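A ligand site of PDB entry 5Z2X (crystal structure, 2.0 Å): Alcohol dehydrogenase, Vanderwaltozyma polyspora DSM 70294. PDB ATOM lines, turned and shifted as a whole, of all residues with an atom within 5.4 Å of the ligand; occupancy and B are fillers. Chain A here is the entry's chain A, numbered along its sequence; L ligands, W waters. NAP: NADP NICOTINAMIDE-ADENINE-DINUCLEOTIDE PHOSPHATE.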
ATOM      1  N   GLY A   7     -10.554  15.640  25.154  1.00  0.00           N
ATOM      2  CA  GLY A   7     -10.312  14.216  25.226  1.00  0.00           C
ATOM      3  C   GLY A   7      -8.875  13.957  25.598  1.00  0.00           C
ATOM      4  O   GLY A   7      -8.150  13.240  24.900  1.00  0.00           O
ATOM      5  N   ALA A   8      -8.425  14.565  26.689  1.00  0.00           N
ATOM      6  CA  ALA A   8      -7.009  14.603  27.033  1.00  0.00           C
ATOM      7  C   ALA A   8      -6.515  13.366  27.778  1.00  0.00           C
ATOM      8  O   ALA A   8      -5.323  13.291  28.077  1.00  0.00           O
ATOM      9  CB  ALA A   8      -6.716  15.857  27.877  1.00  0.00           C
ATOM     10  N   SER A   9      -7.395  12.402  28.082  1.00  0.00           N
ATOM     11  CA  SER A   9      -6.955  11.192  28.777  1.00  0.00           C
ATOM     12  C   SER A   9      -6.606  10.047  27.834  1.00  0.00           C
ATOM     13  O   SER A   9      -6.111   9.017  28.288  1.00  0.00           O
ATOM     14  CB  SER A   9      -8.035  10.723  29.755  1.00  0.00           C
ATOM     15  OG  SER A   9      -9.219  10.391  29.041  1.00  0.00           O
ATOM     16  N   GLY A  10      -6.853  10.207  26.539  1.00  0.00           N
ATOM     17  CA  GLY A  10      -6.635   9.136  25.589  1.00  0.00           C
ATOM     18  C   GLY A  10      -5.166   8.929  25.216  1.00  0.00           C
ATOM     19  O   GLY A  10      -4.275   9.682  25.599  1.00  0.00           O
ATOM     20  N   TYR A  11      -4.950   7.880  24.419  1.00  0.00           N
ATOM     21  CA  TYR A  11      -3.606   7.420  24.062  1.00  0.00           C
ATOM     22  C   TYR A  11      -2.811   8.486  23.322  1.00  0.00           C
ATOM     23  O   TYR A  11      -1.689   8.829  23.705  1.00  0.00           O
ATOM     24  CB  TYR A  11      -3.732   6.145  23.221  1.00  0.00           C
ATOM     25  CG  TYR A  11      -2.520   5.702  22.414  1.00  0.00           C
ATOM     26  CD1 TYR A  11      -1.313   5.382  23.032  1.00  0.00           C
ATOM     27  CD2 TYR A  11      -2.621   5.531  21.034  1.00  0.00           C
ATOM     28  CE1 TYR A  11      -0.217   4.920  22.278  1.00  0.00           C
ATOM     29  CE2 TYR A  11      -1.542   5.070  20.277  1.00  0.00           C
ATOM     30  CZ  TYR A  11      -0.345   4.768  20.895  1.00  0.00           C
ATOM     31  OH  TYR A  11       0.722   4.324  20.116  1.00  0.00           O
ATOM     32  N   ILE A  12      -3.395   9.018  22.251  1.00  0.00           N
ATOM     33  CA  ILE A  12      -2.720  10.029  21.445  1.00  0.00           C
ATOM     34  C   ILE A  12      -2.622  11.334  22.220  1.00  0.00           C
ATOM     35  O   ILE A  12      -1.577  11.990  22.237  1.00  0.00           O
ATOM     36  CB  ILE A  12      -3.474  10.236  20.126  1.00  0.00           C
ATOM     37  CG1 ILE A  12      -3.337   8.994  19.235  1.00  0.00           C
ATOM     38  CG2 ILE A  12      -2.932  11.458  19.390  1.00  0.00           C
ATOM     39  CD1 ILE A  12      -4.256   9.040  17.998  1.00  0.00           C
ATOM     40  N   ALA A  13      -3.720  11.738  22.861  1.00  0.00           N
ATOM     41  CA  ALA A  13      -3.751  13.039  23.508  1.00  0.00           C
ATOM     42  C   ALA A  13      -2.728  13.143  24.630  1.00  0.00           C
ATOM     43  O   ALA A  13      -2.185  14.217  24.872  1.00  0.00           O
ATOM     44  CB  ALA A  13      -5.161  13.325  24.026  1.00  0.00           C
ATOM     45  N   ARG A  32     -13.504  13.156  31.133  1.00  0.00           N
ATOM     46  CA  ARG A  32     -14.885  12.839  31.474  1.00  0.00           C
ATOM     47  C   ARG A  32     -15.190  12.989  32.962  1.00  0.00           C
ATOM     48  O   ARG A  32     -16.368  13.141  33.311  1.00  0.00           O
ATOM     49  CB  ARG A  32     -15.214  11.416  31.026  1.00  0.00           C
ATOM     50  CG  ARG A  32     -15.446  11.217  29.515  1.00  0.00           C
ATOM     51  CD  ARG A  32     -16.330   9.974  29.357  1.00  0.00           C
ATOM     52  NE  ARG A  32     -16.304   9.336  28.034  1.00  0.00           N
ATOM     53  CZ  ARG A  32     -17.372   9.252  27.238  1.00  0.00           C
ATOM     54  NH1 ARG A  32     -17.304   8.625  26.081  1.00  0.00           N
ATOM     55  NH2 ARG A  32     -18.532   9.793  27.601  1.00  0.00           N
ATOM     56  N   LYS A  36     -10.558  10.853  36.543  1.00  0.00           N
ATOM     57  CA  LYS A  36      -9.490  10.788  35.561  1.00  0.00           C
ATOM     58  C   LYS A  36      -8.588  12.006  35.619  1.00  0.00           C
ATOM     59  O   LYS A  36      -7.376  11.884  35.422  1.00  0.00           O
ATOM     60  CB  LYS A  36     -10.089  10.601  34.160  1.00  0.00           C
ATOM     61  CG  LYS A  36     -10.764   9.247  34.009  1.00  0.00           C
ATOM     62  CD  LYS A  36     -11.804   9.202  32.890  1.00  0.00           C
ATOM     63  CE  LYS A  36     -11.943   7.770  32.342  1.00  0.00           C
ATOM     64  NZ  LYS A  36     -13.142   7.590  31.488  1.00  0.00           N
ATOM     65  N   VAL A  54     -15.568  17.560  30.982  1.00  0.00           N
ATOM     66  CA  VAL A  54     -16.589  17.445  29.959  1.00  0.00           C
ATOM     67  C   VAL A  54     -17.026  15.984  29.908  1.00  0.00           C
ATOM     68  O   VAL A  54     -16.356  15.144  29.300  1.00  0.00           O
ATOM     69  CB  VAL A  54     -16.067  17.922  28.588  1.00  0.00           C
ATOM     70  CG1 VAL A  54     -17.063  17.615  27.445  1.00  0.00           C
ATOM     71  CG2 VAL A  54     -15.768  19.409  28.641  1.00  0.00           C
ATOM     72  N   PRO A  55     -18.122  15.632  30.599  1.00  0.00           N
ATOM     73  CA  PRO A  55     -18.475  14.206  30.729  1.00  0.00           C
ATOM     74  C   PRO A  55     -18.893  13.559  29.424  1.00  0.00           C
ATOM     75  O   PRO A  55     -18.714  12.340  29.281  1.00  0.00           O
ATOM     76  CB  PRO A  55     -19.672  14.222  31.709  1.00  0.00           C
ATOM     77  CG  PRO A  55     -19.654  15.539  32.358  1.00  0.00           C
ATOM     78  CD  PRO A  55     -18.954  16.506  31.430  1.00  0.00           C
ATOM     79  N   GLU A  56     -19.434  14.321  28.480  1.00  0.00           N
ATOM     80  CA  GLU A  56     -20.002  13.716  27.277  1.00  0.00           C
ATOM     81  C   GLU A  56     -19.988  14.756  26.156  1.00  0.00           C
ATOM     82  O   GLU A  56     -20.784  15.697  26.172  1.00  0.00           O
ATOM     83  CB  GLU A  56     -21.421  13.217  27.568  1.00  0.00           C
ATOM     84  CG  GLU A  56     -22.127  12.648  26.375  1.00  0.00           C
ATOM     85  CD  GLU A  56     -21.276  11.601  25.690  1.00  0.00           C
ATOM     86  OE1 GLU A  56     -21.121  10.496  26.279  1.00  0.00           O
ATOM     87  OE2 GLU A  56     -20.743  11.901  24.592  1.00  0.00           O
ATOM     88  N   ILE A  57     -19.097  14.592  25.181  1.00  0.00           N
ATOM     89  CA  ILE A  57     -18.996  15.589  24.119  1.00  0.00           C
ATOM     90  C   ILE A  57     -20.241  15.636  23.263  1.00  0.00           C
ATOM     91  O   ILE A  57     -20.480  16.637  22.567  1.00  0.00           O
ATOM     92  CB  ILE A  57     -17.753  15.370  23.229  1.00  0.00           C
ATOM     93  CG1 ILE A  57     -17.859  14.049  22.452  1.00  0.00           C
ATOM     94  CG2 ILE A  57     -16.462  15.453  24.061  1.00  0.00           C
ATOM     95  CD1 ILE A  57     -16.537  13.691  21.684  1.00  0.00           C
ATOM     96  N   ALA A  58     -21.057  14.581  23.268  1.00  0.00           N
ATOM     97  CA  ALA A  58     -22.281  14.582  22.476  1.00  0.00           C
ATOM     98  C   ALA A  58     -23.363  15.465  23.090  1.00  0.00           C
ATOM     99  O   ALA A  58     -24.315  15.813  22.391  1.00  0.00           O
ATOM    100  CB  ALA A  58     -22.815  13.158  22.313  1.00  0.00           C
ATOM    101  N   ALA A  80      -9.388  16.698  19.897  1.00  0.00           N
ATOM    102  CA  ALA A  80      -8.966  15.317  19.734  1.00  0.00           C
ATOM    103  C   ALA A  80      -9.997  14.314  20.242  1.00  0.00           C
ATOM    104  O   ALA A  80      -9.830  13.111  19.991  1.00  0.00           O
ATOM    105  CB  ALA A  80      -7.622  15.074  20.438  1.00  0.00           C
ATOM    106  N   ALA A  81     -11.064  14.758  20.899  1.00  0.00           N
ATOM    107  CA  ALA A  81     -12.059  13.878  21.501  1.00  0.00           C
ATOM    108  C   ALA A  81     -12.974  13.284  20.432  1.00  0.00           C
ATOM    109  O   ALA A  81     -13.780  13.989  19.816  1.00  0.00           O
ATOM    110  CB  ALA A  81     -12.860  14.644  22.557  1.00  0.00           C
ATOM    111  N   SER A  82     -12.890  11.966  20.259  1.00  0.00           N
ATOM    112  CA  SER A  82     -13.850  11.209  19.456  1.00  0.00           C
ATOM    113  C   SER A  82     -13.651   9.749  19.834  1.00  0.00           C
ATOM    114  O   SER A  82     -12.540   9.364  20.216  1.00  0.00           O
ATOM    115  CB  SER A  82     -13.575  11.410  17.951  1.00  0.00           C
ATOM    116  OG  SER A  82     -14.624  10.935  17.130  1.00  0.00           O
ATOM    117  N   PRO A  83     -14.705   8.928  19.794  1.00  0.00           N
ATOM    118  CA  PRO A  83     -14.602   7.563  20.344  1.00  0.00           C
ATOM    119  C   PRO A  83     -13.964   6.614  19.341  1.00  0.00           C
ATOM    120  O   PRO A  83     -14.365   6.562  18.176  1.00  0.00           O
ATOM    121  CB  PRO A  83     -16.058   7.181  20.618  1.00  0.00           C
ATOM    122  CG  PRO A  83     -16.864   8.025  19.662  1.00  0.00           C
ATOM    123  CD  PRO A  83     -16.111   9.331  19.561  1.00  0.00           C
ATOM    124  N   VAL A  84     -13.007   5.821  19.822  1.00  0.00           N
ATOM    125  CA  VAL A  84     -12.405   4.749  19.053  1.00  0.00           C
ATOM    126  C   VAL A  84     -12.785   3.446  19.743  1.00  0.00           C
ATOM    127  O   VAL A  84     -12.081   2.969  20.636  1.00  0.00           O
ATOM    128  CB  VAL A  84     -10.874   4.886  18.964  1.00  0.00           C
ATOM    129  CG1 VAL A  84     -10.303   3.854  17.993  1.00  0.00           C
ATOM    130  CG2 VAL A  84     -10.497   6.314  18.550  1.00  0.00           C
ATOM    131  N   PRO A  98     -21.483  11.108  18.872  1.00  0.00           N
ATOM    132  CA  PRO A  98     -20.425  11.828  19.615  1.00  0.00           C
ATOM    133  C   PRO A  98     -19.390  12.456  18.709  1.00  0.00           C
ATOM    134  O   PRO A  98     -18.957  13.582  18.974  1.00  0.00           O
ATOM    135  CB  PRO A  98     -19.824  10.720  20.495  1.00  0.00           C
ATOM    136  CG  PRO A  98     -20.880   9.668  20.571  1.00  0.00           C
ATOM    137  CD  PRO A  98     -21.510   9.682  19.218  1.00  0.00           C
ATOM    138  N   THR A 124      -8.254  16.269  15.216  1.00  0.00           N
ATOM    139  CA  THR A 124      -7.833  14.911  14.876  1.00  0.00           C
ATOM    140  C   THR A 124      -8.926  14.274  14.027  1.00  0.00           C
ATOM    141  O   THR A 124      -9.947  13.816  14.562  1.00  0.00           O
ATOM    142  CB  THR A 124      -7.567  14.074  16.122  1.00  0.00           C
ATOM    143  OG1 THR A 124      -6.955  14.899  17.114  1.00  0.00           O
ATOM    144  CG2 THR A 124      -6.611  12.913  15.803  1.00  0.00           C
ATOM    145  N   ALA A 125      -8.748  14.272  12.711  1.00  0.00           N
ATOM    146  CA  ALA A 125      -9.618  13.473  11.868  1.00  0.00           C
ATOM    147  C   ALA A 125      -9.008  12.084  11.813  1.00  0.00           C
ATOM    148  O   ALA A 125      -8.489  11.584  12.826  1.00  0.00           O
ATOM    149  CB  ALA A 125      -9.782  14.104  10.483  1.00  0.00           C
ATOM    150  N   SER A 126      -8.996  11.449  10.632  1.00  0.00           N
ATOM    151  CA  SER A 126      -8.319  10.166  10.525  1.00  0.00           C
ATOM    152  C   SER A 126      -8.004   9.884   9.062  1.00  0.00           C
ATOM    153  O   SER A 126      -8.648  10.417   8.162  1.00  0.00           O
ATOM    154  CB  SER A 126      -9.169   9.023  11.091  1.00  0.00           C
ATOM    155  OG  SER A 126      -8.638   7.761  10.712  1.00  0.00           O
ATOM    156  N   TYR A 127      -7.026   9.023   8.858  1.00  0.00           N
ATOM    157  CA  TYR A 127      -6.895   8.385   7.545  1.00  0.00           C
ATOM    158  C   TYR A 127      -8.223   7.755   7.106  1.00  0.00           C
ATOM    159  O   TYR A 127      -8.505   7.665   5.905  1.00  0.00           O
ATOM    160  CB  TYR A 127      -5.753   7.387   7.642  1.00  0.00           C
ATOM    161  CG  TYR A 127      -5.754   6.171   6.753  1.00  0.00           C
ATOM    162  CD1 TYR A 127      -5.238   6.220   5.458  1.00  0.00           C
ATOM    163  CD2 TYR A 127      -6.221   4.956   7.222  1.00  0.00           C
ATOM    164  CE1 TYR A 127      -5.202   5.082   4.654  1.00  0.00           C
ATOM    165  CE2 TYR A 127      -6.194   3.813   6.437  1.00  0.00           C
ATOM    166  CZ  TYR A 127      -5.673   3.877   5.159  1.00  0.00           C
ATOM    167  OH  TYR A 127      -5.648   2.732   4.388  1.00  0.00           O
ATOM    168  N   TYR A 164     -17.285   3.431  12.462  1.00  0.00           N
ATOM    169  CA  TYR A 164     -16.269   4.300  13.046  1.00  0.00           C
ATOM    170  C   TYR A 164     -15.657   5.206  11.984  1.00  0.00           C
ATOM    171  O   TYR A 164     -15.489   6.413  12.201  1.00  0.00           O
ATOM    172  CB  TYR A 164     -15.160   3.501  13.729  1.00  0.00           C
ATOM    173  CG  TYR A 164     -13.928   4.365  13.952  1.00  0.00           C
ATOM    174  CD1 TYR A 164     -13.874   5.278  15.009  1.00  0.00           C
ATOM    175  CD2 TYR A 164     -12.831   4.293  13.088  1.00  0.00           C
ATOM    176  CE1 TYR A 164     -12.773   6.092  15.206  1.00  0.00           C
ATOM    177  CE2 TYR A 164     -11.694   5.115  13.285  1.00  0.00           C
ATOM    178  CZ  TYR A 164     -11.690   6.012  14.354  1.00  0.00           C
ATOM    179  OH  TYR A 164     -10.615   6.833  14.577  1.00  0.00           O
ATOM    180  N   LYS A 168     -15.762   9.460  11.727  1.00  0.00           N
ATOM    181  CA  LYS A 168     -14.630  10.325  11.424  1.00  0.00           C
ATOM    182  C   LYS A 168     -14.927  11.202  10.219  1.00  0.00           C
ATOM    183  O   LYS A 168     -14.712  12.424  10.244  1.00  0.00           O
ATOM    184  CB  LYS A 168     -13.388   9.463  11.182  1.00  0.00           C
ATOM    185  CG  LYS A 168     -12.805   8.770  12.418  1.00  0.00           C
ATOM    186  CD  LYS A 168     -12.907   9.664  13.651  1.00  0.00           C
ATOM    187  CE  LYS A 168     -11.689  10.589  13.653  1.00  0.00           C
ATOM    188  NZ  LYS A 168     -11.517  11.420  14.887  1.00  0.00           N
ATOM    189  N   HIS A 194      -4.736  13.406   9.952  1.00  0.00           N
ATOM    190  CA  HIS A 194      -5.336  12.140   9.519  1.00  0.00           C
ATOM    191  C   HIS A 194      -4.358  10.992   9.743  1.00  0.00           C
ATOM    192  O   HIS A 194      -3.755  10.482   8.794  1.00  0.00           O
ATOM    193  CB  HIS A 194      -5.770  12.195   8.057  1.00  0.00           C
ATOM    194  CG  HIS A 194      -6.646  13.366   7.751  1.00  0.00           C
ATOM    195  ND1 HIS A 194      -7.965  13.210   7.375  1.00  0.00           N
ATOM    196  CD2 HIS A 194      -6.412  14.690   7.765  1.00  0.00           C
ATOM    197  CE1 HIS A 194      -8.499  14.401   7.160  1.00  0.00           C
ATOM    198  NE2 HIS A 194      -7.580  15.319   7.396  1.00  0.00           N
ATOM    199  N   PRO A 195      -4.249  10.513  10.975  1.00  0.00           N
ATOM    200  CA  PRO A 195      -3.401   9.350  11.235  1.00  0.00           C
ATOM    201  C   PRO A 195      -4.071   8.079  10.748  1.00  0.00           C
ATOM    202  O   PRO A 195      -5.305   7.971  10.756  1.00  0.00           O
ATOM    203  CB  PRO A 195      -3.248   9.332  12.758  1.00  0.00           C
ATOM    204  CG  PRO A 195      -3.852  10.656  13.246  1.00  0.00           C
ATOM    205  CD  PRO A 195      -4.876  11.022  12.208  1.00  0.00           C
ATOM    206  N   SER A 196      -3.255   7.127  10.296  1.00  0.00           N
ATOM    207  CA  SER A 196      -3.718   5.765  10.055  1.00  0.00           C
ATOM    208  C   SER A 196      -3.637   5.008  11.388  1.00  0.00           C
ATOM    209  O   SER A 196      -3.659   5.649  12.439  1.00  0.00           O
ATOM    210  CB  SER A 196      -2.904   5.099   8.945  1.00  0.00           C
ATOM    211  OG  SER A 196      -1.524   5.358   9.102  1.00  0.00           O
ATOM    212  N   PHE A 197      -3.550   3.680  11.387  1.00  0.00           N
ATOM    213  CA  PHE A 197      -3.522   2.962  12.664  1.00  0.00           C
ATOM    214  C   PHE A 197      -2.315   3.387  13.491  1.00  0.00           C
ATOM    215  O   PHE A 197      -1.175   3.282  13.040  1.00  0.00           O
ATOM    216  CB  PHE A 197      -3.519   1.461  12.419  1.00  0.00           C
ATOM    217  CG  PHE A 197      -4.883   0.890  12.202  1.00  0.00           C
ATOM    218  CD1 PHE A 197      -5.492   0.972  10.959  1.00  0.00           C
ATOM    219  CD2 PHE A 197      -5.580   0.314  13.251  1.00  0.00           C
ATOM    220  CE1 PHE A 197      -6.760   0.455  10.762  1.00  0.00           C
ATOM    221  CE2 PHE A 197      -6.850  -0.204  13.067  1.00  0.00           C
ATOM    222  CZ  PHE A 197      -7.442  -0.135  11.819  1.00  0.00           C
ATOM    223  N   VAL A 198      -2.560   3.880  14.717  1.00  0.00           N
ATOM    224  CA  VAL A 198      -1.524   4.531  15.522  1.00  0.00           C
ATOM    225  C   VAL A 198      -0.950   3.523  16.492  1.00  0.00           C
ATOM    226  O   VAL A 198      -1.678   2.953  17.314  1.00  0.00           O
ATOM    227  CB  VAL A 198      -2.072   5.771  16.249  1.00  0.00           C
ATOM    228  CG1 VAL A 198      -0.938   6.443  17.035  1.00  0.00           C
ATOM    229  CG2 VAL A 198      -2.614   6.775  15.247  1.00  0.00           C
ATOM    230  N   ASN A 213      -5.597   0.796  24.651  1.00  0.00           N
ATOM    231  CA  ASN A 213      -6.495   1.450  23.693  1.00  0.00           C
ATOM    232  C   ASN A 213      -6.597   0.590  22.439  1.00  0.00           C
ATOM    233  O   ASN A 213      -5.651  -0.151  22.140  1.00  0.00           O
ATOM    234  CB  ASN A 213      -5.983   2.839  23.333  1.00  0.00           C
ATOM    235  CG  ASN A 213      -4.605   2.799  22.702  1.00  0.00           C
ATOM    236  OD1 ASN A 213      -3.620   2.526  23.390  1.00  0.00           O
ATOM    237  ND2 ASN A 213      -4.525   3.039  21.399  1.00  0.00           N
ATOM    238  N   THR A 215      -6.178   0.596  19.144  1.00  0.00           N
ATOM    239  CA  THR A 215      -5.205   0.317  18.085  1.00  0.00           C
ATOM    240  C   THR A 215      -3.954  -0.356  18.650  1.00  0.00           C
ATOM    241  O   THR A 215      -3.427  -1.287  18.026  1.00  0.00           O
ATOM    242  CB  THR A 215      -4.871   1.572  17.269  1.00  0.00           C
ATOM    243  OG1 THR A 215      -4.298   2.605  18.079  1.00  0.00           O
ATOM    244  CG2 THR A 215      -6.137   2.077  16.550  1.00  0.00           C
HETATM  245  PA  NAP L   1      -8.496   6.761  23.034  1.00  0.00           P
HETATM  246  O1A NAP L   1      -7.278   6.298  23.792  1.00  0.00           O
HETATM  247  O2A NAP L   1      -9.690   5.883  23.269  1.00  0.00           O
HETATM  248  O5B NAP L   1      -8.806   8.342  23.390  1.00  0.00           O
HETATM  249  C5B NAP L   1     -10.076   8.844  23.065  1.00  0.00           C
HETATM  250  C4B NAP L   1     -10.285  10.148  23.893  1.00  0.00           C
HETATM  251  O4B NAP L   1     -11.430  10.733  23.573  1.00  0.00           O
HETATM  252  C3B NAP L   1     -10.393   9.732  25.369  1.00  0.00           C
HETATM  253  O3B NAP L   1      -9.895  10.723  26.179  1.00  0.00           O
HETATM  254  C2B NAP L   1     -11.925   9.617  25.489  1.00  0.00           C
HETATM  255  O2B NAP L   1     -12.237   9.682  26.926  1.00  0.00           O
HETATM  256  C1B NAP L   1     -12.395  10.672  24.840  1.00  0.00           C
HETATM  257  N9A NAP L   1     -13.704  10.407  24.314  1.00  0.00           N
HETATM  258  C8A NAP L   1     -14.135   9.591  23.343  1.00  0.00           C
HETATM  259  N7A NAP L   1     -15.453   9.746  23.239  1.00  0.00           N
HETATM  260  C5A NAP L   1     -15.833  10.668  24.144  1.00  0.00           C
HETATM  261  C6A NAP L   1     -17.082  11.182  24.448  1.00  0.00           C
HETATM  262  N6A NAP L   1     -18.336  10.798  23.819  1.00  0.00           N
HETATM  263  N1A NAP L   1     -17.209  12.108  25.393  1.00  0.00           N
HETATM  264  C2A NAP L   1     -16.107  12.544  26.060  1.00  0.00           C
HETATM  265  N3A NAP L   1     -14.878  12.030  25.767  1.00  0.00           N
HETATM  266  C4A NAP L   1     -14.755  11.089  24.807  1.00  0.00           C
HETATM  267  O3  NAP L   1      -8.267   6.695  21.441  1.00  0.00           O
HETATM  268  PN  NAP L   1      -7.055   7.387  20.575  1.00  0.00           P
HETATM  269  O1N NAP L   1      -6.023   8.081  21.441  1.00  0.00           O
HETATM  270  O2N NAP L   1      -6.483   6.275  19.741  1.00  0.00           O
HETATM  271  O5D NAP L   1      -7.841   8.471  19.622  1.00  0.00           O
HETATM  272  C5D NAP L   1      -7.842   9.836  19.948  1.00  0.00           C
HETATM  273  C4D NAP L   1      -8.201  10.644  18.671  1.00  0.00           C
HETATM  274  O4D NAP L   1      -7.381  10.267  17.702  1.00  0.00           O
HETATM  275  C3D NAP L   1      -9.630  10.311  18.191  1.00  0.00           C
HETATM  276  O3D NAP L   1     -10.216  11.427  17.666  1.00  0.00           O
HETATM  277  C2D NAP L   1      -9.347   9.266  17.096  1.00  0.00           C
HETATM  278  O2D NAP L   1     -10.566   9.120  16.241  1.00  0.00           O
HETATM  279  C1D NAP L   1      -8.272   9.744  16.484  1.00  0.00           C
HETATM  280  N1N NAP L   1      -7.548   8.774  15.679  1.00  0.00           N
HETATM  281  C2N NAP L   1      -6.964   7.669  16.226  1.00  0.00           C
HETATM  282  C3N NAP L   1      -6.295   6.760  15.410  1.00  0.00           C
HETATM  283  C7N NAP L   1      -5.627   5.506  15.993  1.00  0.00           C
HETATM  284  O7N NAP L   1      -5.203   4.666  15.253  1.00  0.00           O
HETATM  285  N7N NAP L   1      -5.528   5.309  17.427  1.00  0.00           N
HETATM  286  C4N NAP L   1      -6.238   6.953  14.064  1.00  0.00           C
HETATM  287  C5N NAP L   1      -6.827   8.056  13.509  1.00  0.00           C
HETATM  288  C6N NAP L   1      -7.473   8.966  14.336  1.00  0.00           C
HETATM  289  P2B NAP L   1     -12.805   8.354  27.714  1.00  0.00           P
HETATM  290  O1X NAP L   1     -11.750   7.318  27.657  1.00  0.00           O
HETATM  291  O2X NAP L   1     -13.039   8.830  29.134  1.00  0.00           O
HETATM  292  O3X NAP L   1     -14.080   7.844  27.092  1.00  0.00           O
HETATM  293  O   HOH W   1     -11.874  11.181  29.669  1.00  0.00           O
HETATM  294  O   HOH W   2     -12.797  13.038  27.375  1.00  0.00           O
HETATM  295  O   HOH W   3      -9.437   3.365  21.854  1.00  0.00           O
HETATM  296  O   HOH W   4     -12.339   5.967  22.659  1.00  0.00           O
HETATM  297  O   HOH W   5     -15.568   6.136  28.071  1.00  0.00           O
HETATM  298  O   HOH W   6     -11.120  14.704  17.072  1.00  0.00           O
HETATM  299  O   HOH W   7      -8.299  12.320  22.341  1.00  0.00           O
HETATM  300  O   HOH W   8     -13.971   6.541  24.726  1.00  0.00           O
HETATM  301  O   HOH W   9      -6.526   5.056  26.077  1.00  0.00           O
HETATM  302  O   HOH W  10     -10.632   5.067  25.660  1.00  0.00           O
HETATM  303  O   HOH W  11      -9.286   7.830  28.384  1.00  0.00           O
HETATM  304  O   HOH W  12      -6.176  10.438  22.728  1.00  0.00           O
HETATM  305  O   HOH W  13      -7.119   3.635  20.031  1.00  0.00           O
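The guanidinium group (NE) of Arg 32 is in salt-bridge range of an oxygen (O3X) of the ligand (2.8 Å).
The backbone NH (N) of Gly 10 is in hydrogen-bond range of an oxygen (O3B) of the ligand (3.1 Å).
OH of Tyr 164 sits at hydrogen-bond distance from O2D of the ligand.
A nitrogen (N7N) of the ligand is in hydrogen-bond range of the side-chain hydroxyl (OG1) of Thr 215, 3.0 Å away.
N6A of the ligand is in hydrogen-bond range of OE2 of Glu 56.
An oxygen (O1A) of the ligand sits at hydrogen-bond distance from the backbone NH (N) of Tyr 11, 2.9 Å away.
The backbone NH (N) of Val 198 sits at hydrogen-bond distance from an oxygen (O7N) of the ligand, at 2.8 Å.
N of Ile 12 is in hydrogen-bond range of O1N of the ligand (2.9 Å).
An oxygen (O3B) of the ligand lies within hydrogen-bond range of the side-chain hydroxyl of Ser 9 (3.0 Å).
The backbone NH (N) of Ile 57 lies within hydrogen-bond range of a nitrogen (N1A) of the ligand, at 3.1 Å.
An oxygen (O2X) of the ligand lies within salt-bridge range of the side-chain amino group (NZ) of Lys 36 (2.7 Å).
An oxygen (O2D) of the ligand sits at hydrogen-bond distance from the side-chain amino group of Lys 168, 2.8 Å away.
O of Ala 80 lies within hydrogen-bond range of O3D of the ligand (2.9 Å).
The backbone carbonyl oxygen (O) of Gly 7 sits at hydrogen-bond distance from an oxygen (O3B) of the ligand (3.3 Å).
Water W5 bridges an oxygen (O3X) of the ligand (2.5 Å) and the guanidinium group of Arg 32 (3.3 Å).
Water W11 lies within hydrogen-bond range of an oxygen (O1X) of the ligand (2.6 Å) and the side-chain hydroxyl of Ser 9 (2.6 Å).
Water W13 lies within hydrogen-bond range of O2N of the ligand, ND2 of Asn 213 and N of Thr 215.
Water W3 bridges O2A of the ligand (2.9 Å) and O of Val 84 (2.9 Å).
Water W7 bridges the backbone carbonyl oxygen of Gly 7 and the backbone carbonyl oxygen of Ala 80.
Water W6 bridges the backbone carbonyl oxygen of Thr 124 (2.9 Å) and an oxygen (O3D) of the ligand (3.5 Å).
The side-chain carboxylate (OE2) of Glu 56 sits at hydrogen-bond distance from the backbone NH (N) of Ala 58, 3.0 Å away.
O of Pro 195 lies within hydrogen-bond range of N of Tyr 127 (2.8 Å).
The guanidinium group (NH2) of Arg 32 sits at hydrogen-bond distance from the backbone carbonyl oxygen (O) of Pro 55, 3.1 Å away.
ND1 of His 194 sits at hydrogen-bond distance from O of Ser 126, at 3.0 Å.
The side-chain amino group (NZ) of Lys 168 is in hydrogen-bond range of the backbone carbonyl oxygen (O) of Thr 124, 2.9 Å away.
OG of Ser 126 lies within hydrogen-bond range of O of Pro 195.
ND2 of Asn 213 sits at hydrogen-bond distance from OG1 of Thr 215, at 3.4 Å.
The side-chain hydroxyl (OG1) of Thr 215 lies within hydrogen-bond range of the backbone carbonyl oxygen (O) of Val 198, 2.8 Å away.
An oxygen (O7N) of the ligand lies close to the backbone carbonyl oxygen (O) of Ser 196, 3.4 Å away.
Ala 81 touches the ligand (CA to O4B, 3.8 Å).
Ser 82 touches the ligand (CB to O3D, 3.4 Å).
N of Pro 83 touches N7A of the ligand (3.6 Å).
Val 84 touches the ligand (CG2 to C2D, 3.5 Å).
Pro 98 touches the ligand (CB to N6A, 3.6 Å).
CG2 of Thr 124 touches O4D of the ligand (3.3 Å).
Ala 125 touches the ligand.
Ser 126 touches the ligand (OG to C5N, 3.3 Å).
O of Pro 195 touches C5N of the ligand, at 3.1 Å.
Phe 197 touches the ligand.
Asn 213 touches the ligand.
Hydrophobic or aromatic side chains within 4 Å of the ligand: Tyr 11, Ile 12, Ile 57, Pro 83, Val 84, Pro 98, Tyr 164, Pro 195 and Val 198.
The nearest printed residue that does not touch the ligand is Ala 8 (4.1 Å).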
